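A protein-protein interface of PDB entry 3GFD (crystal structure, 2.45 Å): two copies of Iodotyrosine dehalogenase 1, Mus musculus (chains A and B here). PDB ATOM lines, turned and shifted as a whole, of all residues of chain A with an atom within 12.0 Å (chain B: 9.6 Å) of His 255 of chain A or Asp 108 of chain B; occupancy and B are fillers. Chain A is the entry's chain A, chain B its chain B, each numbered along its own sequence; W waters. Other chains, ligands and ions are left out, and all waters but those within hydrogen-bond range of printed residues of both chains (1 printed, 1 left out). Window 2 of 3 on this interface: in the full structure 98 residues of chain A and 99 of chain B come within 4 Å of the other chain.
The backbone carbonyl oxygen (O) of Val 251 of chain A sits at hydrogen-bond distance from the backbone NH (N) of Val 103 of chain B (2.7 Å).
The backbone carbonyl oxygen (O) of Val 103 of chain B lies within hydrogen-bond range of the backbone NH (N) of Val 253 of chain A (3.1 Å).
N of His 255 of chain A sits close to OD2 of Asp 106 of chain B.
O of Val 104 of chain B sits at hydrogen-bond distance from N of Leu 155 of chain B (2.8 Å).
The side-chain carboxylate of Asp 106 of chain B sits at hydrogen-bond distance from the backbone NH of Asp 108 of chain B, 3.1 Å away.
OD1 of Asp 108 of chain B lies within salt-bridge range of NZ of Lys 112 of chain B.
Thr 252 of chain A touches Val 103 of chain B.
Thr 252 of chain A touches Lys 105 of chain B (CG2 to CE, 3.9 Å).
Val 104 of chain B touches Val 253 of chain A (CG1 to O, 3.9 Å).
Val 253 of chain A touches Leu 215 of chain B (CG2 to O, 3.8 Å).
OD2 of Asp 106 of chain B touches CB of His 254 of chain A, at 3.6 Å.
Asp 108 of chain B touches His 255 of chain A.
Of the printed residues of chain B, His 254 of chain A touches Asp 106.
Printed residues of chain B within 4 Å of His 255 of chain A: Asp 106 (2.9 Å) and Asp 108 (3.9 Å).
Printed residues of chain A within 4 Å of Val 103 of chain B: Val 251 (2.7 Å), Thr 252 (3.4 Å) and Val 253 (3.1 Å).
Of the printed residues of chain A, Val 104 of chain B touches Val 253 (3.9 Å).
No residue of chain A comes within 4 Å of Pro 107 of chain B.
His 111 of chain B touches none of the printed residues of chain A.
No residue of chain A comes within 4 Å of Lys 112 of chain B.
Printed residues of chain A within 4 Å of Leu 215 of chain B: Val 253 (3.8 Å).
The nearest printed residue of chain B that does not touch Thr 252 of chain A is Val 104 of chain B (5.6 Å).
Hydrophobic or aromatic side chains of chain A within 4 Å of the printed part of chain B: Val 253, His 254 and His 255.
Hydrophobic or aromatic side chains of chain B within 4 Å of the printed part of chain A: Val 103, Val 104 and Leu 215.
Among the printed residues, 9 pairs touch across the chains.
Among the printed residues, no Asp or Glu carboxylate lies within 4 Å of a Lys or Arg side-chain nitrogen of the other chain.
No position is printed for both chains.
Of the 9 pairs that touch across the chains among the printed residues, none has its exchanged pair printed and touching as well.
Water W1 lies within hydrogen-bond range of the backbone carbonyl oxygen (O) of Val 253 of chain A (2.5 Å), the backbone NH (N) of Lys 105 of chain B (3.0 Å) and the backbone NH (N) of Asp 106 of chain B (3.1 Å).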
ATOM      1  N   VAL A 251     -26.045  18.507 -27.036  1.00  0.00           N
ATOM      2  CA  VAL A 251     -24.861  18.266 -26.208  1.00  0.00           C
ATOM      3  C   VAL A 251     -25.050  16.982 -25.385  1.00  0.00           C
ATOM      4  O   VAL A 251     -26.055  16.829 -24.716  1.00  0.00           O
ATOM      5  CB  VAL A 251     -24.585  19.462 -25.225  1.00  0.00           C
ATOM      6  CG1 VAL A 251     -23.307  19.204 -24.446  1.00  0.00           C
ATOM      7  CG2 VAL A 251     -24.441  20.740 -25.972  1.00  0.00           C
ATOM      8  N   THR A 252     -24.094  16.062 -25.440  1.00  0.00           N
ATOM      9  CA  THR A 252     -24.112  14.856 -24.583  1.00  0.00           C
ATOM     10  C   THR A 252     -23.140  15.086 -23.447  1.00  0.00           C
ATOM     11  O   THR A 252     -21.967  15.354 -23.711  1.00  0.00           O
ATOM     12  CB  THR A 252     -23.730  13.603 -25.364  1.00  0.00           C
ATOM     13  OG1 THR A 252     -24.648  13.453 -26.442  1.00  0.00           O
ATOM     14  CG2 THR A 252     -23.817  12.339 -24.505  1.00  0.00           C
ATOM     15  N   VAL A 253     -23.646  15.021 -22.201  1.00  0.00           N
ATOM     16  CA  VAL A 253     -22.850  15.313 -20.987  1.00  0.00           C
ATOM     17  C   VAL A 253     -22.685  14.132 -20.040  1.00  0.00           C
ATOM     18  O   VAL A 253     -23.680  13.539 -19.614  1.00  0.00           O
ATOM     19  CB  VAL A 253     -23.441  16.510 -20.189  1.00  0.00           C
ATOM     20  CG1 VAL A 253     -22.738  16.695 -18.856  1.00  0.00           C
ATOM     21  CG2 VAL A 253     -23.295  17.800 -20.966  1.00  0.00           C
ATOM     22  N   HIS A 254     -21.440  13.798 -19.686  1.00  0.00           N
ATOM     23  CA  HIS A 254     -21.165  12.824 -18.569  1.00  0.00           C
ATOM     24  C   HIS A 254     -20.261  13.443 -17.480  1.00  0.00           C
ATOM     25  O   HIS A 254     -19.916  14.621 -17.577  1.00  0.00           O
ATOM     26  CB  HIS A 254     -20.523  11.561 -19.122  1.00  0.00           C
ATOM     27  CG  HIS A 254     -19.522  11.868 -20.178  1.00  0.00           C
ATOM     28  ND1 HIS A 254     -18.279  12.401 -19.883  1.00  0.00           N
ATOM     29  CD2 HIS A 254     -19.617  11.837 -21.529  1.00  0.00           C
ATOM     30  CE1 HIS A 254     -17.627  12.622 -21.012  1.00  0.00           C
ATOM     31  NE2 HIS A 254     -18.420  12.292 -22.024  1.00  0.00           N
ATOM     32  N   HIS A 255     -19.892  12.655 -16.454  1.00  0.00           N
ATOM     33  CA  HIS A 255     -19.089  13.129 -15.263  1.00  0.00           C
ATOM     34  C   HIS A 255     -17.763  13.856 -15.576  1.00  0.00           C
ATOM     35  O   HIS A 255     -17.019  13.451 -16.466  1.00  0.00           O
ATOM     36  CB  HIS A 255     -18.830  11.969 -14.274  1.00  0.00           C
ATOM     37  CG  HIS A 255     -18.216  10.760 -14.916  1.00  0.00           C
ATOM     38  ND1 HIS A 255     -16.853  10.624 -15.100  1.00  0.00           N
ATOM     39  CD2 HIS A 255     -18.786   9.647 -15.453  1.00  0.00           C
ATOM     40  CE1 HIS A 255     -16.613   9.479 -15.723  1.00  0.00           C
ATOM     41  NE2 HIS A 255     -17.768   8.863 -15.940  1.00  0.00           N
ATOM     42  N   VAL B 103     -28.302  15.929 -23.434  1.00  0.00           N
ATOM     43  CA  VAL B 103     -28.652  14.514 -23.347  1.00  0.00           C
ATOM     44  C   VAL B 103     -27.754  13.884 -22.302  1.00  0.00           C
ATOM     45  O   VAL B 103     -26.532  14.005 -22.379  1.00  0.00           O
ATOM     46  CB  VAL B 103     -28.415  13.837 -24.717  1.00  0.00           C
ATOM     47  CG1 VAL B 103     -28.603  12.297 -24.635  1.00  0.00           C
ATOM     48  CG2 VAL B 103     -29.343  14.466 -25.785  1.00  0.00           C
ATOM     49  N   VAL B 104     -28.344  13.226 -21.315  1.00  0.00           N
ATOM     50  CA  VAL B 104     -27.585  12.592 -20.258  1.00  0.00           C
ATOM     51  C   VAL B 104     -27.981  11.103 -20.228  1.00  0.00           C
ATOM     52  O   VAL B 104     -29.162  10.788 -20.115  1.00  0.00           O
ATOM     53  CB  VAL B 104     -27.896  13.250 -18.894  1.00  0.00           C
ATOM     54  CG1 VAL B 104     -27.051  12.627 -17.784  1.00  0.00           C
ATOM     55  CG2 VAL B 104     -27.665  14.736 -18.947  1.00  0.00           C
ATOM     56  N   LYS B 105     -26.995  10.222 -20.356  1.00  0.00           N
ATOM     57  CA  LYS B 105     -27.140   8.781 -20.254  1.00  0.00           C
ATOM     58  C   LYS B 105     -26.331   8.248 -19.044  1.00  0.00           C
ATOM     59  O   LYS B 105     -26.621   7.189 -18.499  1.00  0.00           O
ATOM     60  CB  LYS B 105     -26.515   8.117 -21.484  1.00  0.00           C
ATOM     61  CG  LYS B 105     -27.192   8.477 -22.785  1.00  0.00           C
ATOM     62  CD  LYS B 105     -26.357   7.939 -23.972  1.00  0.00           C
ATOM     63  CE  LYS B 105     -24.939   8.588 -23.984  1.00  0.00           C
ATOM     64  NZ  LYS B 105     -24.080   8.249 -25.191  1.00  0.00           N
ATOM     65  N   ASP B 106     -25.245   8.923 -18.717  1.00  0.00           N
ATOM     66  CA  ASP B 106     -24.350   8.424 -17.650  1.00  0.00           C
ATOM     67  C   ASP B 106     -25.091   8.250 -16.291  1.00  0.00           C
ATOM     68  O   ASP B 106     -25.724   9.173 -15.813  1.00  0.00           O
ATOM     69  CB  ASP B 106     -23.086   9.311 -17.592  1.00  0.00           C
ATOM     70  CG  ASP B 106     -22.265   9.137 -16.318  1.00  0.00           C
ATOM     71  OD1 ASP B 106     -22.272   8.062 -15.632  1.00  0.00           O
ATOM     72  OD2 ASP B 106     -21.562  10.111 -15.977  1.00  0.00           O
ATOM     73  N   PRO B 107     -25.073   7.036 -15.713  1.00  0.00           N
ATOM     74  CA  PRO B 107     -25.808   6.790 -14.452  1.00  0.00           C
ATOM     75  C   PRO B 107     -25.442   7.679 -13.250  1.00  0.00           C
ATOM     76  O   PRO B 107     -26.341   8.027 -12.462  1.00  0.00           O
ATOM     77  CB  PRO B 107     -25.510   5.320 -14.113  1.00  0.00           C
ATOM     78  CG  PRO B 107     -24.820   4.778 -15.287  1.00  0.00           C
ATOM     79  CD  PRO B 107     -24.442   5.819 -16.251  1.00  0.00           C
ATOM     80  N   ASP B 108     -24.152   7.990 -13.113  1.00  0.00           N
ATOM     81  CA  ASP B 108     -23.639   8.861 -12.066  1.00  0.00           C
ATOM     82  C   ASP B 108     -24.352  10.245 -12.234  1.00  0.00           C
ATOM     83  O   ASP B 108     -25.012  10.755 -11.305  1.00  0.00           O
ATOM     84  CB  ASP B 108     -22.086   8.889 -12.192  1.00  0.00           C
ATOM     85  CG  ASP B 108     -21.424  10.088 -11.501  1.00  0.00           C
ATOM     86  OD1 ASP B 108     -21.784  11.224 -11.874  1.00  0.00           O
ATOM     87  OD2 ASP B 108     -20.497   9.941 -10.637  1.00  0.00           O
ATOM     88  N   MET B 109     -24.233  10.810 -13.431  1.00  0.00           N
ATOM     89  CA  MET B 109     -24.818  12.094 -13.735  1.00  0.00           C
ATOM     90  C   MET B 109     -26.354  12.083 -13.634  1.00  0.00           C
ATOM     91  O   MET B 109     -26.950  13.031 -13.099  1.00  0.00           O
ATOM     92  CB  MET B 109     -24.329  12.573 -15.110  1.00  0.00           C
ATOM     93  CG  MET B 109     -24.831  13.950 -15.530  1.00  0.00           C
ATOM     94  SD  MET B 109     -24.408  15.216 -14.336  1.00  0.00           S
ATOM     95  CE  MET B 109     -22.764  15.654 -14.879  1.00  0.00           C
ATOM     96  N   LYS B 110     -27.008  11.023 -14.112  1.00  0.00           N
ATOM     97  CA  LYS B 110     -28.499  10.934 -13.960  1.00  0.00           C
ATOM     98  C   LYS B 110     -28.880  10.940 -12.483  1.00  0.00           C
ATOM     99  O   LYS B 110     -29.900  11.518 -12.092  1.00  0.00           O
ATOM    100  CB  LYS B 110     -29.159   9.730 -14.630  1.00  0.00           C
ATOM    101  CG  LYS B 110     -29.030   9.666 -16.156  1.00  0.00           C
ATOM    102  CD  LYS B 110     -29.819   8.457 -16.692  1.00  0.00           C
ATOM    103  CE  LYS B 110     -29.356   7.122 -16.055  1.00  0.00           C
ATOM    104  NZ  LYS B 110     -30.013   5.929 -16.683  1.00  0.00           N
ATOM    105  N   HIS B 111     -28.063  10.326 -11.653  1.00  0.00           N
ATOM    106  CA  HIS B 111     -28.430  10.256 -10.265  1.00  0.00           C
ATOM    107  C   HIS B 111     -28.225  11.582  -9.502  1.00  0.00           C
ATOM    108  O   HIS B 111     -29.030  11.923  -8.629  1.00  0.00           O
ATOM    109  CB  HIS B 111     -27.744   9.104  -9.547  1.00  0.00           C
ATOM    110  CG  HIS B 111     -28.323   8.860  -8.204  1.00  0.00           C
ATOM    111  ND1 HIS B 111     -27.655   9.179  -7.034  1.00  0.00           N
ATOM    112  CD2 HIS B 111     -29.530   8.363  -7.834  1.00  0.00           C
ATOM    113  CE1 HIS B 111     -28.423   8.876  -6.000  1.00  0.00           C
ATOM    114  NE2 HIS B 111     -29.569   8.393  -6.456  1.00  0.00           N
ATOM    115  N   LYS B 112     -27.170  12.320  -9.848  1.00  0.00           N
ATOM    116  CA  LYS B 112     -26.968  13.674  -9.350  1.00  0.00           C
ATOM    117  C   LYS B 112     -28.119  14.590  -9.734  1.00  0.00           C
ATOM    118  O   LYS B 112     -28.574  15.395  -8.916  1.00  0.00           O
ATOM    119  CB  LYS B 112     -25.661  14.235  -9.861  1.00  0.00           C
ATOM    120  CG  LYS B 112     -24.486  13.613  -9.156  1.00  0.00           C
ATOM    121  CD  LYS B 112     -23.216  13.949  -9.896  1.00  0.00           C
ATOM    122  CE  LYS B 112     -22.030  13.860  -8.967  1.00  0.00           C
ATOM    123  NZ  LYS B 112     -20.965  13.064  -9.647  1.00  0.00           N
ATOM    124  N   ILE B 113     -28.589  14.484 -10.968  1.00  0.00           N
ATOM    125  CA  ILE B 113     -29.761  15.218 -11.387  1.00  0.00           C
ATOM    126  C   ILE B 113     -30.950  14.818 -10.495  1.00  0.00           C
ATOM    127  O   ILE B 113     -31.661  15.677  -9.991  1.00  0.00           O
ATOM    128  CB  ILE B 113     -30.052  14.939 -12.879  1.00  0.00           C
ATOM    129  CG1 ILE B 113     -28.981  15.602 -13.767  1.00  0.00           C
ATOM    130  CG2 ILE B 113     -31.468  15.400 -13.299  1.00  0.00           C
ATOM    131  CD1 ILE B 113     -29.155  15.234 -15.239  1.00  0.00           C
ATOM    132  N   ARG B 114     -31.128  13.525 -10.249  1.00  0.00           N
ATOM    133  CA  ARG B 114     -32.171  13.066  -9.362  1.00  0.00           C
ATOM    134  C   ARG B 114     -32.032  13.649  -7.942  1.00  0.00           C
ATOM    135  O   ARG B 114     -33.032  14.082  -7.342  1.00  0.00           O
ATOM    136  CB  ARG B 114     -32.207  11.548  -9.311  1.00  0.00           C
ATOM    137  CG  ARG B 114     -33.244  11.033  -8.314  1.00  0.00           C
ATOM    138  CD  ARG B 114     -33.460   9.579  -8.429  1.00  0.00           C
ATOM    139  NE  ARG B 114     -34.595   9.168  -7.611  1.00  0.00           N
ATOM    140  CZ  ARG B 114     -34.820   7.907  -7.228  1.00  0.00           C
ATOM    141  NH1 ARG B 114     -34.002   6.924  -7.619  1.00  0.00           N
ATOM    142  NH2 ARG B 114     -35.891   7.619  -6.496  1.00  0.00           N
ATOM    143  N   GLU B 115     -30.823  13.681  -7.391  1.00  0.00           N
ATOM    144  CA  GLU B 115     -30.679  14.249  -6.040  1.00  0.00           C
ATOM    145  C   GLU B 115     -31.100  15.715  -5.992  1.00  0.00           C
ATOM    146  O   GLU B 115     -31.757  16.131  -5.058  1.00  0.00           O
ATOM    147  CB  GLU B 115     -29.262  14.141  -5.526  1.00  0.00           C
ATOM    148  CG  GLU B 115     -28.848  12.728  -5.220  1.00  0.00           C
ATOM    149  CD  GLU B 115     -27.356  12.631  -4.887  1.00  0.00           C
ATOM    150  OE1 GLU B 115     -26.543  13.498  -5.319  1.00  0.00           O
ATOM    151  OE2 GLU B 115     -26.990  11.671  -4.193  1.00  0.00           O
ATOM    152  N   ILE B 116     -30.744  16.490  -7.007  1.00  0.00           N
ATOM    153  CA  ILE B 116     -31.138  17.877  -7.010  1.00  0.00           C
ATOM    154  C   ILE B 116     -32.660  17.999  -7.128  1.00  0.00           C
ATOM    155  O   ILE B 116     -33.287  18.767  -6.410  1.00  0.00           O
ATOM    156  CB  ILE B 116     -30.471  18.626  -8.173  1.00  0.00           C
ATOM    157  CG1 ILE B 116     -28.958  18.752  -7.909  1.00  0.00           C
ATOM    158  CG2 ILE B 116     -31.195  19.970  -8.431  1.00  0.00           C
ATOM    159  CD1 ILE B 116     -28.177  19.036  -9.202  1.00  0.00           C
ATOM    160  N   LEU B 149     -35.797   9.379 -13.080  1.00  0.00           N
ATOM    161  CA  LEU B 149     -34.542  10.087 -13.365  1.00  0.00           C
ATOM    162  C   LEU B 149     -33.361   9.102 -13.330  1.00  0.00           C
ATOM    163  O   LEU B 149     -32.365   9.296 -14.051  1.00  0.00           O
ATOM    164  CB  LEU B 149     -34.303  11.267 -12.395  1.00  0.00           C
ATOM    165  CG  LEU B 149     -35.338  12.391 -12.546  1.00  0.00           C
ATOM    166  CD1 LEU B 149     -35.236  13.399 -11.396  1.00  0.00           C
ATOM    167  CD2 LEU B 149     -35.198  13.078 -13.920  1.00  0.00           C
ATOM    168  N   ASP B 150     -33.467   8.048 -12.515  1.00  0.00           N
ATOM    169  CA  ASP B 150     -32.485   6.962 -12.561  1.00  0.00           C
ATOM    170  C   ASP B 150     -32.810   5.942 -13.650  1.00  0.00           C
ATOM    171  O   ASP B 150     -31.929   5.538 -14.400  1.00  0.00           O
ATOM    172  CB  ASP B 150     -32.339   6.252 -11.207  1.00  0.00           C
ATOM    173  CG  ASP B 150     -31.387   6.983 -10.268  1.00  0.00           C
ATOM    174  OD1 ASP B 150     -30.384   7.576 -10.767  1.00  0.00           O
ATOM    175  OD2 ASP B 150     -31.642   6.986  -9.032  1.00  0.00           O
ATOM    176  N   LEU B 155     -31.945  11.121 -20.428  1.00  0.00           N
ATOM    177  CA  LEU B 155     -32.696  12.314 -20.017  1.00  0.00           C
ATOM    178  C   LEU B 155     -32.367  13.397 -21.042  1.00  0.00           C
ATOM    179  O   LEU B 155     -31.194  13.551 -21.435  1.00  0.00           O
ATOM    180  CB  LEU B 155     -32.315  12.792 -18.605  1.00  0.00           C
ATOM    181  CG  LEU B 155     -32.323  11.757 -17.492  1.00  0.00           C
ATOM    182  CD1 LEU B 155     -31.760  12.311 -16.167  1.00  0.00           C
ATOM    183  CD2 LEU B 155     -33.729  11.196 -17.320  1.00  0.00           C
ATOM    184  N   LEU B 214     -24.440  22.091 -12.917  1.00  0.00           N
ATOM    185  CA  LEU B 214     -23.979  20.704 -12.856  1.00  0.00           C
ATOM    186  C   LEU B 214     -23.620  20.221 -14.244  1.00  0.00           C
ATOM    187  O   LEU B 214     -22.628  19.506 -14.452  1.00  0.00           O
ATOM    188  CB  LEU B 214     -25.080  19.814 -12.259  1.00  0.00           C
ATOM    189  CG  LEU B 214     -24.831  18.304 -12.335  1.00  0.00           C
ATOM    190  CD1 LEU B 214     -23.766  17.802 -11.274  1.00  0.00           C
ATOM    191  CD2 LEU B 214     -26.141  17.533 -12.242  1.00  0.00           C
ATOM    192  N   LEU B 215     -24.420  20.621 -15.220  1.00  0.00           N
ATOM    193  CA  LEU B 215     -24.204  20.132 -16.571  1.00  0.00           C
ATOM    194  C   LEU B 215     -23.238  21.014 -17.388  1.00  0.00           C
ATOM    195  O   LEU B 215     -23.083  20.790 -18.591  1.00  0.00           O
ATOM    196  CB  LEU B 215     -25.533  19.999 -17.284  1.00  0.00           C
ATOM    197  CG  LEU B 215     -26.374  18.717 -17.186  1.00  0.00           C
ATOM    198  CD1 LEU B 215     -25.754  17.586 -16.403  1.00  0.00           C
ATOM    199  CD2 LEU B 215     -27.825  18.972 -16.792  1.00  0.00           C
ATOM    200  N   GLY B 216     -22.586  21.997 -16.747  1.00  0.00           N
ATOM    201  CA  GLY B 216     -21.587  22.818 -17.433  1.00  0.00           C
ATOM    202  C   GLY B 216     -22.189  23.770 -18.474  1.00  0.00           C
ATOM    203  O   GLY B 216     -21.466  24.223 -19.347  1.00  0.00           O
HETATM  204  O   HOH W   1     -24.220  11.260 -20.405  1.00  0.00           O
